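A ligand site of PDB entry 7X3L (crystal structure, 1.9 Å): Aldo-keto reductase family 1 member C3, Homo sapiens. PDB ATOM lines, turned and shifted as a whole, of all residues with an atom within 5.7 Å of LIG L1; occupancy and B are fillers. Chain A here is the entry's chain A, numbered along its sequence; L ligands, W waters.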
ATOM      1  N   TYR A  30      -5.553 -24.309  10.772  1.00  0.00           N
ATOM      2  CA  TYR A  30      -6.597 -23.997  11.735  1.00  0.00           C
ATOM      3  C   TYR A  30      -7.475 -25.211  11.983  1.00  0.00           C
ATOM      4  O   TYR A  30      -7.941 -25.857  11.044  1.00  0.00           O
ATOM      5  CB  TYR A  30      -7.493 -22.849  11.287  1.00  0.00           C
ATOM      6  CG  TYR A  30      -8.578 -22.596  12.323  1.00  0.00           C
ATOM      7  CD1 TYR A  30      -8.272 -22.000  13.532  1.00  0.00           C
ATOM      8  CD2 TYR A  30      -9.886 -23.000  12.101  1.00  0.00           C
ATOM      9  CE1 TYR A  30      -9.242 -21.794  14.499  1.00  0.00           C
ATOM     10  CE2 TYR A  30     -10.871 -22.785  13.065  1.00  0.00           C
ATOM     11  CZ  TYR A  30     -10.542 -22.178  14.256  1.00  0.00           C
ATOM     12  OH  TYR A  30     -11.491 -21.968  15.224  1.00  0.00           O
ATOM     13  N   LEU A  60      -4.131 -16.366  16.347  1.00  0.00           N
ATOM     14  CA  LEU A  60      -5.519 -16.690  16.669  1.00  0.00           C
ATOM     15  C   LEU A  60      -5.757 -18.201  16.799  1.00  0.00           C
ATOM     16  O   LEU A  60      -6.627 -18.631  17.572  1.00  0.00           O
ATOM     17  CB  LEU A  60      -6.430 -16.110  15.588  1.00  0.00           C
ATOM     18  CG  LEU A  60      -7.935 -16.384  15.741  1.00  0.00           C
ATOM     19  CD1 LEU A  60      -8.552 -15.550  16.836  1.00  0.00           C
ATOM     20  CD2 LEU A  60      -8.630 -16.140  14.404  1.00  0.00           C
ATOM     21  N   TYR A  61      -4.983 -19.020  16.066  1.00  0.00           N
ATOM     22  CA  TYR A  61      -5.294 -20.440  15.947  1.00  0.00           C
ATOM     23  C   TYR A  61      -4.951 -21.240  17.197  1.00  0.00           C
ATOM     24  O   TYR A  61      -5.303 -22.428  17.277  1.00  0.00           O
ATOM     25  CB  TYR A  61      -4.557 -21.056  14.751  1.00  0.00           C
ATOM     26  CG  TYR A  61      -4.846 -20.407  13.410  1.00  0.00           C
ATOM     27  CD1 TYR A  61      -5.863 -19.469  13.273  1.00  0.00           C
ATOM     28  CD2 TYR A  61      -4.072 -20.713  12.282  1.00  0.00           C
ATOM     29  CE1 TYR A  61      -6.114 -18.858  12.052  1.00  0.00           C
ATOM     30  CE2 TYR A  61      -4.324 -20.118  11.046  1.00  0.00           C
ATOM     31  CZ  TYR A  61      -5.349 -19.175  10.949  1.00  0.00           C
ATOM     32  OH  TYR A  61      -5.601 -18.572   9.749  1.00  0.00           O
ATOM     33  N   LYS A  90       0.336 -14.485  11.715  1.00  0.00           N
ATOM     34  CA  LYS A  90      -0.581 -13.375  11.497  1.00  0.00           C
ATOM     35  C   LYS A  90      -0.777 -12.591  12.786  1.00  0.00           C
ATOM     36  O   LYS A  90      -0.945 -13.163  13.867  1.00  0.00           O
ATOM     37  CB  LYS A  90      -1.942 -13.877  10.987  1.00  0.00           C
ATOM     38  CG  LYS A  90      -1.860 -14.826   9.776  1.00  0.00           C
ATOM     39  CD  LYS A  90      -3.207 -14.929   9.062  1.00  0.00           C
ATOM     40  CE  LYS A  90      -3.199 -16.073   8.062  1.00  0.00           C
ATOM     41  NZ  LYS A  90      -3.120 -17.401   8.776  1.00  0.00           N
ATOM     42  N   TRP A  92      -2.913 -10.659  15.261  1.00  0.00           N
ATOM     43  CA  TRP A  92      -4.339 -10.663  15.553  1.00  0.00           C
ATOM     44  C   TRP A  92      -4.843  -9.229  15.775  1.00  0.00           C
ATOM     45  O   TRP A  92      -4.075  -8.323  16.067  1.00  0.00           O
ATOM     46  CB  TRP A  92      -4.665 -11.577  16.752  1.00  0.00           C
ATOM     47  CG  TRP A  92      -6.135 -11.636  16.993  1.00  0.00           C
ATOM     48  CD1 TRP A  92      -6.791 -11.339  18.153  1.00  0.00           C
ATOM     49  CD2 TRP A  92      -7.148 -11.914  16.010  1.00  0.00           C
ATOM     50  NE1 TRP A  92      -8.151 -11.448  17.959  1.00  0.00           N
ATOM     51  CE2 TRP A  92      -8.398 -11.800  16.662  1.00  0.00           C
ATOM     52  CE3 TRP A  92      -7.120 -12.273  14.657  1.00  0.00           C
ATOM     53  CZ2 TRP A  92      -9.602 -12.015  16.007  1.00  0.00           C
ATOM     54  CZ3 TRP A  92      -8.324 -12.488  14.002  1.00  0.00           C
ATOM     55  CH2 TRP A  92      -9.552 -12.355  14.672  1.00  0.00           C
ATOM     56  N   SER A  93      -6.155  -9.048  15.593  1.00  0.00           N
ATOM     57  CA  SER A  93      -6.803  -7.750  15.491  1.00  0.00           C
ATOM     58  C   SER A  93      -6.828  -6.955  16.792  1.00  0.00           C
ATOM     59  O   SER A  93      -7.131  -5.751  16.760  1.00  0.00           O
ATOM     60  CB  SER A  93      -8.228  -7.949  14.983  1.00  0.00           C
ATOM     61  OG  SER A  93      -8.224  -8.766  13.812  1.00  0.00           O
ATOM     62  N   HIS A 123      -3.909  -9.995  10.105  1.00  0.00           N
ATOM     63  CA  HIS A 123      -4.895 -11.055   9.923  1.00  0.00           C
ATOM     64  C   HIS A 123      -6.183 -10.529   9.309  1.00  0.00           C
ATOM     65  O   HIS A 123      -6.801 -11.189   8.463  1.00  0.00           O
ATOM     66  CB  HIS A 123      -5.190 -11.737  11.275  1.00  0.00           C
ATOM     67  CG  HIS A 123      -5.716 -13.126  11.154  1.00  0.00           C
ATOM     68  ND1 HIS A 123      -5.400 -14.119  12.065  1.00  0.00           N
ATOM     69  CD2 HIS A 123      -6.567 -13.689  10.265  1.00  0.00           C
ATOM     70  CE1 HIS A 123      -6.020 -15.235  11.722  1.00  0.00           C
ATOM     71  NE2 HIS A 123      -6.729 -15.001  10.631  1.00  0.00           N
ATOM     72  N   SER A 124      -6.591  -9.319   9.686  1.00  0.00           N
ATOM     73  CA  SER A 124      -7.871  -8.767   9.294  1.00  0.00           C
ATOM     74  C   SER A 124      -7.834  -7.253   9.469  1.00  0.00           C
ATOM     75  O   SER A 124      -7.115  -6.762  10.357  1.00  0.00           O
ATOM     76  CB  SER A 124      -8.986  -9.393  10.155  1.00  0.00           C
ATOM     77  OG  SER A 124     -10.123  -8.553  10.290  1.00  0.00           O
ATOM     78  N   PRO A 125      -8.562  -6.493   8.648  1.00  0.00           N
ATOM     79  CA  PRO A 125      -8.653  -5.038   8.904  1.00  0.00           C
ATOM     80  C   PRO A 125      -9.590  -4.665  10.027  1.00  0.00           C
ATOM     81  O   PRO A 125      -9.692  -3.479  10.351  1.00  0.00           O
ATOM     82  CB  PRO A 125      -9.176  -4.484   7.570  1.00  0.00           C
ATOM     83  CG  PRO A 125     -10.033  -5.613   7.042  1.00  0.00           C
ATOM     84  CD  PRO A 125      -9.344  -6.898   7.471  1.00  0.00           C
ATOM     85  N   MET A 126     -10.317  -5.634  10.603  1.00  0.00           N
ATOM     86  CA  MET A 126     -11.369  -5.325  11.569  1.00  0.00           C
ATOM     87  C   MET A 126     -10.781  -5.268  12.973  1.00  0.00           C
ATOM     88  O   MET A 126     -10.815  -6.242  13.727  1.00  0.00           O
ATOM     89  CB  MET A 126     -12.506  -6.351  11.469  1.00  0.00           C
ATOM     90  CG  MET A 126     -13.259  -6.261  10.130  1.00  0.00           C
ATOM     91  SD  MET A 126     -14.545  -7.519   9.980  1.00  0.00           S
ATOM     92  CE  MET A 126     -13.584  -9.004   9.751  1.00  0.00           C
ATOM     93  N   ASN A 173      -7.560 -10.439   4.237  1.00  0.00           N
ATOM     94  CA  ASN A 173      -8.942  -9.988   4.279  1.00  0.00           C
ATOM     95  C   ASN A 173      -9.102  -8.496   3.948  1.00  0.00           C
ATOM     96  O   ASN A 173     -10.107  -7.894   4.319  1.00  0.00           O
ATOM     97  CB  ASN A 173      -9.585 -10.306   5.627  1.00  0.00           C
ATOM     98  CG  ASN A 173      -9.675 -11.787   5.876  1.00  0.00           C
ATOM     99  OD1 ASN A 173     -10.354 -12.511   5.133  1.00  0.00           O
ATOM    100  ND2 ASN A 173      -8.973 -12.266   6.891  1.00  0.00           N
ATOM    101  N   TYR A 222      -7.781 -18.738   0.855  1.00  0.00           N
ATOM    102  CA  TYR A 222      -8.185 -19.599   1.959  1.00  0.00           C
ATOM    103  C   TYR A 222      -9.625 -20.043   1.768  1.00  0.00           C
ATOM    104  O   TYR A 222     -10.379 -19.480   0.961  1.00  0.00           O
ATOM    105  CB  TYR A 222      -7.994 -18.925   3.327  1.00  0.00           C
ATOM    106  CG  TYR A 222      -8.957 -17.819   3.749  1.00  0.00           C
ATOM    107  CD1 TYR A 222     -10.298 -18.089   4.040  1.00  0.00           C
ATOM    108  CD2 TYR A 222      -8.493 -16.518   3.921  1.00  0.00           C
ATOM    109  CE1 TYR A 222     -11.146 -17.096   4.479  1.00  0.00           C
ATOM    110  CE2 TYR A 222      -9.356 -15.493   4.353  1.00  0.00           C
ATOM    111  CZ  TYR A 222     -10.679 -15.796   4.626  1.00  0.00           C
ATOM    112  OH  TYR A 222     -11.544 -14.818   5.068  1.00  0.00           O
ATOM    113  N   ARG A 232     -20.538 -21.762  13.909  1.00  0.00           N
ATOM    114  CA  ARG A 232     -20.531 -20.412  14.466  1.00  0.00           C
ATOM    115  C   ARG A 232     -20.696 -19.348  13.398  1.00  0.00           C
ATOM    116  O   ARG A 232     -21.251 -18.282  13.668  1.00  0.00           O
ATOM    117  CB  ARG A 232     -19.231 -20.178  15.240  1.00  0.00           C
ATOM    118  CG  ARG A 232     -19.131 -20.973  16.541  1.00  0.00           C
ATOM    119  CD  ARG A 232     -17.731 -20.874  17.125  1.00  0.00           C
ATOM    120  NE  ARG A 232     -16.755 -21.636  16.356  1.00  0.00           N
ATOM    121  CZ  ARG A 232     -15.448 -21.603  16.577  1.00  0.00           C
ATOM    122  NH1 ARG A 232     -14.960 -20.831  17.542  1.00  0.00           N
ATOM    123  NH2 ARG A 232     -14.618 -22.315  15.825  1.00  0.00           N
ATOM    124  N   TRP A 233     -20.227 -19.605  12.169  1.00  0.00           N
ATOM    125  CA  TRP A 233     -20.234 -18.573  11.130  1.00  0.00           C
ATOM    126  C   TRP A 233     -20.768 -19.000   9.781  1.00  0.00           C
ATOM    127  O   TRP A 233     -21.014 -18.129   8.939  1.00  0.00           O
ATOM    128  CB  TRP A 233     -18.823 -18.036  10.892  1.00  0.00           C
ATOM    129  CG  TRP A 233     -18.050 -17.805  12.117  1.00  0.00           C
ATOM    130  CD1 TRP A 233     -18.230 -16.808  13.033  1.00  0.00           C
ATOM    131  CD2 TRP A 233     -16.942 -18.570  12.567  1.00  0.00           C
ATOM    132  NE1 TRP A 233     -17.298 -16.913  14.029  1.00  0.00           N
ATOM    133  CE2 TRP A 233     -16.494 -17.996  13.771  1.00  0.00           C
ATOM    134  CE3 TRP A 233     -16.275 -19.687  12.068  1.00  0.00           C
ATOM    135  CZ2 TRP A 233     -15.425 -18.499  14.486  1.00  0.00           C
ATOM    136  CZ3 TRP A 233     -15.215 -20.194  12.786  1.00  0.00           C
ATOM    137  CH2 TRP A 233     -14.801 -19.601  13.977  1.00  0.00           C
ATOM    138  N   PHE A 312     -18.205 -17.278   5.401  1.00  0.00           N
ATOM    139  CA  PHE A 312     -18.200 -16.662   6.729  1.00  0.00           C
ATOM    140  C   PHE A 312     -19.128 -15.459   6.691  1.00  0.00           C
ATOM    141  O   PHE A 312     -18.847 -14.453   6.021  1.00  0.00           O
ATOM    142  CB  PHE A 312     -16.785 -16.263   7.137  1.00  0.00           C
ATOM    143  CG  PHE A 312     -15.850 -17.429   7.228  1.00  0.00           C
ATOM    144  CD1 PHE A 312     -15.168 -17.854   6.100  1.00  0.00           C
ATOM    145  CD2 PHE A 312     -15.655 -18.099   8.425  1.00  0.00           C
ATOM    146  CE1 PHE A 312     -14.303 -18.925   6.159  1.00  0.00           C
ATOM    147  CE2 PHE A 312     -14.783 -19.181   8.489  1.00  0.00           C
ATOM    148  CZ  PHE A 312     -14.103 -19.589   7.344  1.00  0.00           C
ATOM    149  N   PHE A 317     -19.313  -9.468  12.010  1.00  0.00           N
ATOM    150  CA  PHE A 317     -18.402  -8.930  11.006  1.00  0.00           C
ATOM    151  C   PHE A 317     -19.021  -7.722  10.303  1.00  0.00           C
ATOM    152  O   PHE A 317     -18.404  -6.657  10.208  1.00  0.00           O
ATOM    153  CB  PHE A 317     -18.040  -9.994   9.970  1.00  0.00           C
ATOM    154  CG  PHE A 317     -17.498 -11.271  10.554  1.00  0.00           C
ATOM    155  CD1 PHE A 317     -16.552 -11.239  11.570  1.00  0.00           C
ATOM    156  CD2 PHE A 317     -17.937 -12.495  10.081  1.00  0.00           C
ATOM    157  CE1 PHE A 317     -16.053 -12.427  12.096  1.00  0.00           C
ATOM    158  CE2 PHE A 317     -17.438 -13.683  10.607  1.00  0.00           C
ATOM    159  CZ  PHE A 317     -16.496 -13.649  11.615  1.00  0.00           C
ATOM    160  N   TYR A 323     -15.309  -3.775   7.831  1.00  0.00           N
ATOM    161  CA  TYR A 323     -15.790  -4.983   7.178  1.00  0.00           C
ATOM    162  C   TYR A 323     -15.453  -4.914   5.680  1.00  0.00           C
ATOM    163  O   TYR A 323     -15.775  -3.912   5.027  1.00  0.00           O
ATOM    164  CB  TYR A 323     -17.305  -5.106   7.388  1.00  0.00           C
ATOM    165  CG  TYR A 323     -17.993  -6.312   6.756  1.00  0.00           C
ATOM    166  CD1 TYR A 323     -17.651  -7.613   7.120  1.00  0.00           C
ATOM    167  CD2 TYR A 323     -19.030  -6.124   5.857  1.00  0.00           C
ATOM    168  CE1 TYR A 323     -18.317  -8.702   6.567  1.00  0.00           C
ATOM    169  CE2 TYR A 323     -19.702  -7.202   5.298  1.00  0.00           C
ATOM    170  CZ  TYR A 323     -19.345  -8.487   5.659  1.00  0.00           C
ATOM    171  OH  TYR A 323     -20.016  -9.541   5.096  1.00  0.00           O
ATOM    172  N   PRO A 324     -14.772  -5.910   5.127  1.00  0.00           N
ATOM    173  CA  PRO A 324     -14.284  -5.796   3.740  1.00  0.00           C
ATOM    174  C   PRO A 324     -15.322  -6.100   2.670  1.00  0.00           C
ATOM    175  O   PRO A 324     -15.063  -5.813   1.499  1.00  0.00           O
ATOM    176  CB  PRO A 324     -13.142  -6.810   3.692  1.00  0.00           C
ATOM    177  CG  PRO A 324     -13.504  -7.831   4.695  1.00  0.00           C
ATOM    178  CD  PRO A 324     -14.202  -7.089   5.816  1.00  0.00           C
ATOM    179  N   TYR A 325     -16.480  -6.665   3.007  1.00  0.00           N
ATOM    180  CA  TYR A 325     -17.439  -7.021   1.975  1.00  0.00           C
ATOM    181  C   TYR A 325     -18.544  -5.970   1.890  1.00  0.00           C
ATOM    182  O   TYR A 325     -18.589  -5.022   2.669  1.00  0.00           O
ATOM    183  CB  TYR A 325     -18.037  -8.406   2.258  1.00  0.00           C
ATOM    184  CG  TYR A 325     -16.994  -9.520   2.356  1.00  0.00           C
ATOM    185  CD1 TYR A 325     -15.854  -9.499   1.577  1.00  0.00           C
ATOM    186  CD2 TYR A 325     -17.180 -10.581   3.251  1.00  0.00           C
ATOM    187  CE1 TYR A 325     -14.896 -10.541   1.669  1.00  0.00           C
ATOM    188  CE2 TYR A 325     -16.237 -11.599   3.357  1.00  0.00           C
ATOM    189  CZ  TYR A 325     -15.101 -11.576   2.569  1.00  0.00           C
ATOM    190  OH  TYR A 325     -14.180 -12.581   2.688  1.00  0.00           O
HETATM  191  C1  LIG L   1     -13.188 -11.872   7.369  1.00  0.00           C
HETATM  192  C2  LIG L   1     -12.425 -12.859   7.948  1.00  0.00           C
HETATM  193  C3  LIG L   1     -13.036 -13.909   8.630  1.00  0.00           C
HETATM  194  C4  LIG L   1     -15.374 -10.782   6.777  1.00  0.00           C
HETATM  195  C5  LIG L   1     -12.230 -14.985   9.266  1.00  0.00           C
HETATM  196  C6  LIG L   1     -11.788 -17.375   9.450  1.00  0.00           C
HETATM  197  C7  LIG L   1     -11.288 -14.757  10.282  1.00  0.00           C
HETATM  198  C8  LIG L   1     -10.053 -18.280  11.070  1.00  0.00           C
HETATM  199  C9  LIG L   1     -10.922 -19.475  11.446  1.00  0.00           C
HETATM  200  C10 LIG L   1     -14.426 -13.922   8.683  1.00  0.00           C
HETATM  201  C11 LIG L   1     -10.830 -17.139  10.425  1.00  0.00           C
HETATM  202  C12 LIG L   1     -10.607 -15.827  10.833  1.00  0.00           C
HETATM  203  C13 LIG L   1     -10.961 -13.390  10.803  1.00  0.00           C
HETATM  204  C14 LIG L   1      -8.814 -18.620  10.234  1.00  0.00           C
HETATM  205  C15 LIG L   1     -11.799 -19.152  12.617  1.00  0.00           C
HETATM  206  C16 LIG L   1     -15.186 -12.921   8.095  1.00  0.00           C
HETATM  207  C17 LIG L   1     -14.561 -11.870   7.419  1.00  0.00           C
HETATM  208  C18 LIG L   1     -12.475 -16.309   8.878  1.00  0.00           C
HETATM  209  F1  LIG L   1     -12.554 -10.868   6.732  1.00  0.00           F
HETATM  210  F2  LIG L   1     -10.133 -12.718  10.003  1.00  0.00           F
HETATM  211  F3  LIG L   1     -12.025 -12.615  10.976  1.00  0.00           F
HETATM  212  F4  LIG L   1     -10.359 -13.427  11.978  1.00  0.00           F
HETATM  213  O1  LIG L   1      -8.025 -17.697   9.981  1.00  0.00           O
HETATM  214  O2  LIG L   1      -8.657 -19.812   9.870  1.00  0.00           O
HETATM  215  P1  LG2 L   2     -10.296 -25.583   3.551  1.00  0.00           P
HETATM  216  O1  LG2 L   2     -11.297 -24.849   2.673  1.00  0.00           O
HETATM  217  O2  LG2 L   2      -8.857 -25.528   2.992  1.00  0.00           O
HETATM  218  O3  LG2 L   2     -10.752 -27.143   3.773  1.00  0.00           O
HETATM  219  C1  LG2 L   2     -12.075 -27.376   4.261  1.00  0.00           C
HETATM  220  C2  LG2 L   2     -12.203 -28.892   4.496  1.00  0.00           C
HETATM  221  O4  LG2 L   2     -11.821 -29.531   3.386  1.00  0.00           O
HETATM  222  C3  LG2 L   2     -11.163 -29.309   5.536  1.00  0.00           C
HETATM  223  O5  LG2 L   2     -11.734 -29.294   6.770  1.00  0.00           O
HETATM  224  C4  LG2 L   2     -10.847 -30.783   5.085  1.00  0.00           C
HETATM  225  O6  LG2 L   2     -11.470 -31.699   6.096  1.00  0.00           O
HETATM  226  C5  LG2 L   2     -11.396 -30.984   3.908  1.00  0.00           C
HETATM  227  N1  LG2 L   2     -10.441 -31.522   2.972  1.00  0.00           N
HETATM  228  C6  LG2 L   2      -9.125 -31.297   2.841  1.00  0.00           C
HETATM  229  N2  LG2 L   2      -8.668 -32.035   1.804  1.00  0.00           N
HETATM  230  C7  LG2 L   2      -9.715 -32.727   1.283  1.00  0.00           C
HETATM  231  C8  LG2 L   2      -9.783 -33.610   0.244  1.00  0.00           C
HETATM  232  N3  LG2 L   2      -8.704 -34.064  -0.615  1.00  0.00           N
HETATM  233  N4  LG2 L   2     -10.961 -34.175  -0.085  1.00  0.00           N
HETATM  234  C9  LG2 L   2     -12.084 -33.857   0.619  1.00  0.00           C
HETATM  235  N5  LG2 L   2     -12.020 -32.980   1.671  1.00  0.00           N
HETATM  236  C10 LG2 L   2     -10.820 -32.411   2.002  1.00  0.00           C
HETATM  237  O7  LG2 L   2     -10.332 -25.059   5.126  1.00  0.00           O
HETATM  238  P2  LG2 L   2     -10.161 -23.583   5.730  1.00  0.00           P
HETATM  239  O8  LG2 L   2      -9.730 -23.794   7.147  1.00  0.00           O
HETATM  240  O9  LG2 L   2     -11.444 -22.837   5.658  1.00  0.00           O
HETATM  241  O10 LG2 L   2      -8.950 -22.800   4.912  1.00  0.00           O
HETATM  242  C11 LG2 L   2      -7.608 -23.408   4.914  1.00  0.00           C
HETATM  243  C12 LG2 L   2      -6.610 -22.578   5.761  1.00  0.00           C
HETATM  244  O11 LG2 L   2      -6.601 -21.325   5.350  1.00  0.00           O
HETATM  245  C13 LG2 L   2      -7.019 -22.518   7.250  1.00  0.00           C
HETATM  246  O12 LG2 L   2      -6.698 -23.673   7.963  1.00  0.00           O
HETATM  247  C14 LG2 L   2      -6.183 -21.287   7.645  1.00  0.00           C
HETATM  248  O13 LG2 L   2      -4.750 -21.759   7.687  1.00  0.00           O
HETATM  249  C15 LG2 L   2      -6.344 -20.428   6.656  1.00  0.00           C
HETATM  250  N6  LG2 L   2      -7.450 -19.477   6.830  1.00  0.00           N
HETATM  251  C16 LG2 L   2      -7.146 -18.150   6.961  1.00  0.00           C
HETATM  252  C17 LG2 L   2      -8.167 -17.221   7.156  1.00  0.00           C
HETATM  253  C18 LG2 L   2      -7.836 -15.756   7.312  1.00  0.00           C
HETATM  254  O14 LG2 L   2      -8.627 -15.031   7.854  1.00  0.00           O
HETATM  255  N7  LG2 L   2      -6.557 -15.273   6.801  1.00  0.00           N
HETATM  256  C19 LG2 L   2      -9.465 -17.609   7.210  1.00  0.00           C
HETATM  257  C20 LG2 L   2      -9.769 -18.927   7.058  1.00  0.00           C
HETATM  258  C21 LG2 L   2      -8.752 -19.854   6.854  1.00  0.00           C
HETATM  259  P3  LG2 L   2     -10.477 -32.791   6.821  1.00  0.00           P
HETATM  260  O15 LG2 L   2      -9.604 -32.120   7.810  1.00  0.00           O
HETATM  261  O16 LG2 L   2     -11.400 -33.789   7.508  1.00  0.00           O
HETATM  262  O17 LG2 L   2      -9.625 -33.465   5.782  1.00  0.00           O
HETATM  263  O   HOH W   1     -10.579 -21.698   9.064  1.00  0.00           O
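An oxygen (O14) of LG2 L2 lies within hydrogen-bond range of the side-chain amide nitrogen (ND2) of Asn 173.
An oxygen (O12) of LG2 L2 lies within hydrogen-bond range of the backbone NH (N) of Tyr 30 (3.1 Å).
A ring nitrogen (NE2) of His 123 lies within hydrogen-bond range of an oxygen (O14) of LG2 L2, 3.4 Å away.
An oxygen (O1) of LIG L1 lies within hydrogen-bond range of a ring nitrogen (NE2) of His 123, 3.1 Å away.
An oxygen (O1) of LIG L1 sits at hydrogen-bond distance from the side-chain hydroxyl (OH) of Tyr 61 (2.6 Å).
The side-chain amide oxygen (OD1) of Asn 173 sits close to a fluorine (F1) of LIG L1.
Residues that only touch LIG L1: Tyr 30 (3.5 Å), Trp 92 (3.0 Å), Ser 124 (3.5 Å), Met 126 (3.7 Å), Tyr 222 (3.6 Å), Trp 233 (3.3 Å), Phe 312 (3.6 Å), Phe 317 (3.4 Å), Tyr 323 (3.6 Å), Pro 324 (3.8 Å) and Tyr 325 (3.6 Å).
Hydrophobic or aromatic side chains that line LIG L1: Tyr 30, Tyr 61, Trp 92, His 123, Met 126, Trp 233, Phe 312, Phe 317, Tyr 323, Pro 324 and Tyr 325.
Water W1 bridges an oxygen (O2) of LIG L1 (2.8 Å) and an oxygen (O8) of LG2 L2 (3.0 Å).
O of His 123 sits at hydrogen-bond distance from ND2 of Asn 173, at 2.9 Å.
The side-chain amide oxygen of Asn 173 lies within hydrogen-bond range of the side-chain hydroxyl of Tyr 222 (2.6 Å).
N of Met 126 is in hydrogen-bond range of OG of Ser 124 (2.9 Å).
OH of Tyr 30 is in hydrogen-bond range of NH2 of Arg 232 (3.2 Å).
The side-chain amino group of Lys 90 sits at hydrogen-bond distance from the side-chain hydroxyl of Tyr 61 (2.9 Å).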
